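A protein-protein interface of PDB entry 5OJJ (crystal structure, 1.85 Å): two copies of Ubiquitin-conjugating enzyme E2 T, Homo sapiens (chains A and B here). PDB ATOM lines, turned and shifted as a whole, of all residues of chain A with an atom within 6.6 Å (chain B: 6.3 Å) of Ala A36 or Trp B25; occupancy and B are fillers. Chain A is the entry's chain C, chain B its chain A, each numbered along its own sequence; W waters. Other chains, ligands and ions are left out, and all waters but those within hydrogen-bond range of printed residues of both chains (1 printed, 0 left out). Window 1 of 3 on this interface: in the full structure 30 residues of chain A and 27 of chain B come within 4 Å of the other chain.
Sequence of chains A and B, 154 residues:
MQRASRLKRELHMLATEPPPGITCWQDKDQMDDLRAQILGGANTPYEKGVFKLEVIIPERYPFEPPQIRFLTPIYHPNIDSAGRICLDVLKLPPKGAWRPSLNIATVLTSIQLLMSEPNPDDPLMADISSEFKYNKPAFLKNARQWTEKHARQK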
ATOM      1  N   ASP A  33      -8.570  33.540  24.491  1.00  0.00           N
ATOM      2  CA  ASP A  33      -8.384  33.604  23.040  1.00  0.00           C
ATOM      3  C   ASP A  33      -6.915  33.824  22.610  1.00  0.00           C
ATOM      4  O   ASP A  33      -6.635  34.167  21.452  1.00  0.00           O
ATOM      5  CB  ASP A  33      -9.335  34.668  22.432  1.00  0.00           C
ATOM      6  CG  ASP A  33      -9.108  36.088  22.986  1.00  0.00           C
ATOM      7  OD1 ASP A  33      -9.605  37.047  22.346  1.00  0.00           O
ATOM      8  OD2 ASP A  33      -8.474  36.263  24.058  1.00  0.00           O
ATOM      9  N   LEU A  34      -5.977  33.578  23.528  1.00  0.00           N
ATOM     10  CA  LEU A  34      -4.545  33.568  23.198  1.00  0.00           C
ATOM     11  C   LEU A  34      -4.155  32.267  22.489  1.00  0.00           C
ATOM     12  O   LEU A  34      -4.589  31.187  22.893  1.00  0.00           O
ATOM     13  CB  LEU A  34      -3.671  33.693  24.464  1.00  0.00           C
ATOM     14  CG  LEU A  34      -2.787  34.908  24.708  1.00  0.00           C
ATOM     15  CD1 LEU A  34      -1.794  34.544  25.808  1.00  0.00           C
ATOM     16  CD2 LEU A  34      -2.044  35.408  23.473  1.00  0.00           C
ATOM     17  N   ARG A  35      -3.313  32.387  21.471  1.00  0.00           N
ATOM     18  CA  ARG A  35      -2.778  31.233  20.722  1.00  0.00           C
ATOM     19  C   ARG A  35      -1.246  31.331  20.570  1.00  0.00           C
ATOM     20  O   ARG A  35      -0.690  32.424  20.567  1.00  0.00           O
ATOM     21  CB  ARG A  35      -3.415  31.165  19.342  1.00  0.00           C
ATOM     22  CG  ARG A  35      -4.935  31.088  19.328  1.00  0.00           C
ATOM     23  CD  ARG A  35      -5.490  29.783  19.877  1.00  0.00           C
ATOM     24  NE  ARG A  35      -6.958  29.830  19.913  1.00  0.00           N
ATOM     25  CZ  ARG A  35      -7.722  30.170  20.959  1.00  0.00           C
ATOM     26  NH1 ARG A  35      -7.206  30.491  22.147  1.00  0.00           N
ATOM     27  NH2 ARG A  35      -9.046  30.183  20.810  1.00  0.00           N
ATOM     28  N   ALA A  36      -0.595  30.181  20.432  1.00  0.00           N
ATOM     29  CA  ALA A  36       0.842  30.072  20.200  1.00  0.00           C
ATOM     30  C   ALA A  36       1.145  29.061  19.098  1.00  0.00           C
ATOM     31  O   ALA A  36       0.299  28.202  18.776  1.00  0.00           O
ATOM     32  CB  ALA A  36       1.552  29.666  21.484  1.00  0.00           C
ATOM     33  N   GLN A  37       2.349  29.175  18.534  1.00  0.00           N
ATOM     34  CA  GLN A  37       2.892  28.248  17.536  1.00  0.00           C
ATOM     35  C   GLN A  37       4.349  27.924  17.893  1.00  0.00           C
ATOM     36  O   GLN A  37       5.127  28.842  18.180  1.00  0.00           O
ATOM     37  CB  GLN A  37       2.837  28.877  16.139  1.00  0.00           C
ATOM     38  CG  GLN A  37       3.483  28.094  15.012  1.00  0.00           C
ATOM     39  CD  GLN A  37       3.429  28.845  13.680  1.00  0.00           C
ATOM     40  OE1 GLN A  37       2.372  28.926  13.045  1.00  0.00           O
ATOM     41  NE2 GLN A  37       4.572  29.394  13.249  1.00  0.00           N
ATOM     42  N   ILE A  38       4.701  26.636  17.847  1.00  0.00           N
ATOM     43  CA  ILE A  38       6.088  26.157  18.022  1.00  0.00           C
ATOM     44  C   ILE A  38       6.526  25.379  16.777  1.00  0.00           C
ATOM     45  O   ILE A  38       5.826  24.460  16.326  1.00  0.00           O
ATOM     46  CB  ILE A  38       6.242  25.251  19.270  1.00  0.00           C
ATOM     47  CG1 ILE A  38       5.752  25.986  20.528  1.00  0.00           C
ATOM     48  CG2 ILE A  38       7.695  24.794  19.453  1.00  0.00           C
ATOM     49  CD1 ILE A  38       5.674  25.119  21.767  1.00  0.00           C
ATOM     50  N   PHE A  51       3.380  23.578  14.988  1.00  0.00           N
ATOM     51  CA  PHE A  51       2.428  23.092  16.009  1.00  0.00           C
ATOM     52  C   PHE A  51       1.681  24.241  16.684  1.00  0.00           C
ATOM     53  O   PHE A  51       2.283  25.087  17.321  1.00  0.00           O
ATOM     54  CB  PHE A  51       3.133  22.198  17.042  1.00  0.00           C
ATOM     55  CG  PHE A  51       3.718  20.934  16.447  1.00  0.00           C
ATOM     56  CD1 PHE A  51       5.004  20.930  15.902  1.00  0.00           C
ATOM     57  CD2 PHE A  51       2.968  19.754  16.405  1.00  0.00           C
ATOM     58  CE1 PHE A  51       5.533  19.770  15.329  1.00  0.00           C
ATOM     59  CE2 PHE A  51       3.494  18.600  15.848  1.00  0.00           C
ATOM     60  CZ  PHE A  51       4.777  18.608  15.300  1.00  0.00           C
ATOM     61  N   LYS A  52       0.365  24.281  16.497  1.00  0.00           N
ATOM     62  CA  LYS A  52      -0.493  25.288  17.103  1.00  0.00           C
ATOM     63  C   LYS A  52      -0.971  24.849  18.488  1.00  0.00           C
ATOM     64  O   LYS A  52      -1.283  23.655  18.710  1.00  0.00           O
ATOM     65  CB  LYS A  52      -1.699  25.597  16.211  1.00  0.00           C
ATOM     66  CG  LYS A  52      -2.449  26.867  16.625  1.00  0.00           C
ATOM     67  CD  LYS A  52      -3.577  27.232  15.679  1.00  0.00           C
ATOM     68  CE  LYS A  52      -4.176  28.586  16.019  1.00  0.00           C
ATOM     69  NZ  LYS A  52      -5.436  28.833  15.266  1.00  0.00           N
ATOM     70  N   LEU A  53      -1.026  25.829  19.403  1.00  0.00           N
ATOM     71  CA  LEU A  53      -1.502  25.661  20.778  1.00  0.00           C
ATOM     72  C   LEU A  53      -2.515  26.718  21.225  1.00  0.00           C
ATOM     73  O   LEU A  53      -2.523  27.851  20.717  1.00  0.00           O
ATOM     74  CB  LEU A  53      -0.322  25.712  21.768  1.00  0.00           C
ATOM     75  CG  LEU A  53       0.807  24.720  21.471  1.00  0.00           C
ATOM     76  CD1 LEU A  53       1.938  25.396  20.713  1.00  0.00           C
ATOM     77  CD2 LEU A  53       1.336  24.087  22.748  1.00  0.00           C
ATOM     78  N   GLU A  54      -3.349  26.316  22.192  1.00  0.00           N
ATOM     79  CA  GLU A  54      -4.265  27.180  22.947  1.00  0.00           C
ATOM     80  C   GLU A  54      -3.636  27.589  24.303  1.00  0.00           C
ATOM     81  O   GLU A  54      -3.152  26.727  25.025  1.00  0.00           O
ATOM     82  CB  GLU A  54      -5.577  26.403  23.179  1.00  0.00           C
ATOM     83  CG  GLU A  54      -6.616  27.045  24.086  1.00  0.00           C
ATOM     84  CD  GLU A  54      -7.803  26.117  24.370  1.00  0.00           C
ATOM     85  OE1 GLU A  54      -7.680  25.160  25.173  1.00  0.00           O
ATOM     86  OE2 GLU A  54      -8.875  26.358  23.790  1.00  0.00           O
ATOM     87  N   VAL A  55      -3.669  28.884  24.649  1.00  0.00           N
ATOM     88  CA  VAL A  55      -3.135  29.383  25.933  1.00  0.00           C
ATOM     89  C   VAL A  55      -4.257  30.122  26.666  1.00  0.00           C
ATOM     90  O   VAL A  55      -4.699  31.185  26.207  1.00  0.00           O
ATOM     91  CB  VAL A  55      -1.915  30.327  25.741  1.00  0.00           C
ATOM     92  CG1 VAL A  55      -1.252  30.662  27.086  1.00  0.00           C
ATOM     93  CG2 VAL A  55      -0.872  29.739  24.790  1.00  0.00           C
ATOM     94  N   ILE A  68      -2.443  25.289  29.026  1.00  0.00           N
ATOM     95  CA  ILE A  68      -1.990  25.138  27.647  1.00  0.00           C
ATOM     96  C   ILE A  68      -2.294  23.716  27.136  1.00  0.00           C
ATOM     97  O   ILE A  68      -1.972  22.740  27.811  1.00  0.00           O
ATOM     98  CB  ILE A  68      -0.477  25.456  27.508  1.00  0.00           C
ATOM     99  CG1 ILE A  68      -0.162  26.847  28.129  1.00  0.00           C
ATOM    100  CG2 ILE A  68      -0.040  25.374  26.051  1.00  0.00           C
ATOM    101  CD1 ILE A  68       1.228  27.387  27.874  1.00  0.00           C
ATOM    102  N   LEU A  71      -3.372  22.222  20.001  1.00  0.00           N
ATOM    103  CA  LEU A  71      -4.486  22.116  19.036  1.00  0.00           C
ATOM    104  C   LEU A  71      -4.099  21.188  17.867  1.00  0.00           C
ATOM    105  O   LEU A  71      -4.934  20.427  17.371  1.00  0.00           O
ATOM    106  CB  LEU A  71      -4.898  23.501  18.506  1.00  0.00           C
ATOM    107  CG  LEU A  71      -5.414  24.518  19.533  1.00  0.00           C
ATOM    108  CD1 LEU A  71      -5.708  25.856  18.866  1.00  0.00           C
ATOM    109  CD2 LEU A  71      -6.632  24.023  20.289  1.00  0.00           C
ATOM    110  N   LEU A 108       6.344  28.188  27.306  1.00  0.00           N
ATOM    111  CA  LEU A 108       6.414  27.817  25.897  1.00  0.00           C
ATOM    112  C   LEU A 108       7.798  27.247  25.539  1.00  0.00           C
ATOM    113  O   LEU A 108       7.888  26.236  24.854  1.00  0.00           O
ATOM    114  CB  LEU A 108       6.036  28.987  24.976  1.00  0.00           C
ATOM    115  CG  LEU A 108       4.581  29.485  25.037  1.00  0.00           C
ATOM    116  CD1 LEU A 108       4.376  30.767  24.259  1.00  0.00           C
ATOM    117  CD2 LEU A 108       3.566  28.450  24.543  1.00  0.00           C
ATOM    118  N   ILE B  22       9.217  30.335  18.328  1.00  0.00           N
ATOM    119  CA  ILE B  22       7.939  30.473  19.032  1.00  0.00           C
ATOM    120  C   ILE B  22       7.265  31.807  18.646  1.00  0.00           C
ATOM    121  O   ILE B  22       7.944  32.830  18.529  1.00  0.00           O
ATOM    122  CB  ILE B  22       8.143  30.357  20.572  1.00  0.00           C
ATOM    123  CG1 ILE B  22       8.677  28.948  20.892  1.00  0.00           C
ATOM    124  CG2 ILE B  22       6.827  30.630  21.315  1.00  0.00           C
ATOM    125  CD1 ILE B  22       9.111  28.657  22.304  1.00  0.00           C
ATOM    126  N   THR B  23       5.941  31.790  18.440  1.00  0.00           N
ATOM    127  CA  THR B  23       5.124  33.014  18.302  1.00  0.00           C
ATOM    128  C   THR B  23       3.857  32.897  19.189  1.00  0.00           C
ATOM    129  O   THR B  23       3.452  31.784  19.523  1.00  0.00           O
ATOM    130  CB  THR B  23       4.761  33.283  16.827  1.00  0.00           C
ATOM    131  OG1 THR B  23       4.215  32.097  16.229  1.00  0.00           O
ATOM    132  CG2 THR B  23       6.006  33.712  16.023  1.00  0.00           C
ATOM    133  N   CYS B  24       3.277  34.031  19.614  1.00  0.00           N
ATOM    134  CA  CYS B  24       2.110  34.044  20.523  1.00  0.00           C
ATOM    135  C   CYS B  24       1.277  35.275  20.209  1.00  0.00           C
ATOM    136  O   CYS B  24       1.803  36.394  20.245  1.00  0.00           O
ATOM    137  CB  CYS B  24       2.492  34.003  22.025  1.00  0.00           C
ATOM    138  SG  CYS B  24       1.067  33.941  23.214  1.00  0.00           S
ATOM    139  N   TRP B  25       0.005  35.056  19.854  1.00  0.00           N
ATOM    140  CA  TRP B  25      -0.893  36.108  19.363  1.00  0.00           C
ATOM    141  C   TRP B  25      -2.343  35.874  19.791  1.00  0.00           C
ATOM    142  O   TRP B  25      -2.700  34.800  20.253  1.00  0.00           O
ATOM    143  CB  TRP B  25      -0.835  36.214  17.821  1.00  0.00           C
ATOM    144  CG  TRP B  25      -1.483  35.059  17.098  1.00  0.00           C
ATOM    145  CD1 TRP B  25      -2.740  35.024  16.553  1.00  0.00           C
ATOM    146  CD2 TRP B  25      -0.919  33.765  16.876  1.00  0.00           C
ATOM    147  NE1 TRP B  25      -2.986  33.795  16.011  1.00  0.00           N
ATOM    148  CE2 TRP B  25      -1.884  33.000  16.190  1.00  0.00           C
ATOM    149  CE3 TRP B  25       0.312  33.176  17.189  1.00  0.00           C
ATOM    150  CZ2 TRP B  25      -1.664  31.675  15.822  1.00  0.00           C
ATOM    151  CZ3 TRP B  25       0.537  31.861  16.813  1.00  0.00           C
ATOM    152  CH2 TRP B  25      -0.445  31.122  16.132  1.00  0.00           C
ATOM    153  N   GLN B  26      -3.172  36.906  19.622  1.00  0.00           N
ATOM    154  CA  GLN B  26      -4.594  36.850  20.019  1.00  0.00           C
ATOM    155  C   GLN B  26      -5.490  36.584  18.784  1.00  0.00           C
ATOM    156  O   GLN B  26      -5.412  37.335  17.823  1.00  0.00           O
ATOM    157  CB  GLN B  26      -4.967  38.184  20.678  1.00  0.00           C
ATOM    158  CG  GLN B  26      -5.749  38.079  21.971  1.00  0.00           C
ATOM    159  CD  GLN B  26      -5.832  39.395  22.753  1.00  0.00           C
ATOM    160  OE1 GLN B  26      -6.921  39.809  23.136  1.00  0.00           O
ATOM    161  NE2 GLN B  26      -4.686  40.038  23.013  1.00  0.00           N
ATOM    162  N   ASP B  27      -6.307  35.522  18.824  1.00  0.00           N
ATOM    163  CA  ASP B  27      -7.347  35.217  17.806  1.00  0.00           C
ATOM    164  C   ASP B  27      -8.715  35.810  18.213  1.00  0.00           C
ATOM    165  O   ASP B  27      -9.037  35.874  19.389  1.00  0.00           O
ATOM    166  CB  ASP B  27      -7.535  33.692  17.642  1.00  0.00           C
ATOM    167  CG  ASP B  27      -6.847  33.124  16.420  1.00  0.00           C
ATOM    168  OD1 ASP B  27      -5.766  33.611  16.030  1.00  0.00           O
ATOM    169  OD2 ASP B  27      -7.387  32.147  15.856  1.00  0.00           O
HETATM  170  O   HOH W   1       6.523  29.818  15.636  1.00  0.00           O
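NE1 of Trp B25 sits at hydrogen-bond distance from OD1 of Asp B27, at 2.8 Å.
The backbone carbonyl oxygen of Lys A52 is in hydrogen-bond range of the backbone NH of Leu A71, at 2.8 Å.
The backbone carbonyl oxygen of Ala A36 sits at hydrogen-bond distance from the backbone NH of Leu A53.
N of Val A55 lies within hydrogen-bond range of O of Leu A34, at 3.0 Å.
Among the printed residues, pairs that only touch across the chains: Asp A33 with Gln B26, Leu A34 with Cys B24, Leu A34 with Trp B25, Ala A36 with Thr B23, Ala A36 with Trp B25, Gln A37 with Ile B22, Gln A37 with Trp B25, Lys A52 with Trp B25 and Leu A108 with Ile B22.
No position is printed for both chains.
Of the 14 pairs that touch across the chains among the printed residues, none has its exchanged pair printed and touching as well.
Of the 14 printed residues of chain A, 7 touch a printed residue of chain B.
Hydrophobic or aromatic side chains of chain A within 4 Å of the printed part of chain B: Leu A34, Ala A36 and Leu A108.
Among the printed residues, Asp or Glu carboxylates within 4 Å of a Lys or Arg side-chain nitrogen of the other chain: Lys A52 with Asp B27.
Water W1 bridges O of Gln A37 (3.1 Å) and OG1 of Thr B23 (3.3 Å).
Ala A36 touches just these residues of chain B: Thr B23 (3.2 Å) and Trp B25 (3.7 Å).
Of the printed residues of chain B, Lys A52 touches Trp B25 and Asp B27.
Of the printed residues of chain A, Asp B27 touches Asp A33 (3.0 Å) and Lys A52 (3.9 Å).
Val A55 touches none of the printed residues of chain B.
Ile A68 touches none of the printed residues of chain B.
The nearest printed residue of chain A that does not touch Trp B25 is Asp A33 (4.2 Å).
O of Thr B23 sits at hydrogen-bond distance from N of Gln A37 (3.0 Å).
The backbone NH (N) of Arg A35 is in hydrogen-bond range of the backbone carbonyl oxygen (O) of Trp B25, at 2.8 Å.
The side-chain carboxylate (OD2) of Asp B27 lies within salt-bridge range of the side-chain amino group (NZ) of Lys A52, 3.9 Å away.
The side-chain sulfur (SG) of Cys B24 lies close to the backbone carbonyl oxygen (O) of Arg A35 (3.5 Å).
The backbone NH (N) of Asp B27 sits at hydrogen-bond distance from the backbone carbonyl oxygen (O) of Asp A33 (3.0 Å).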
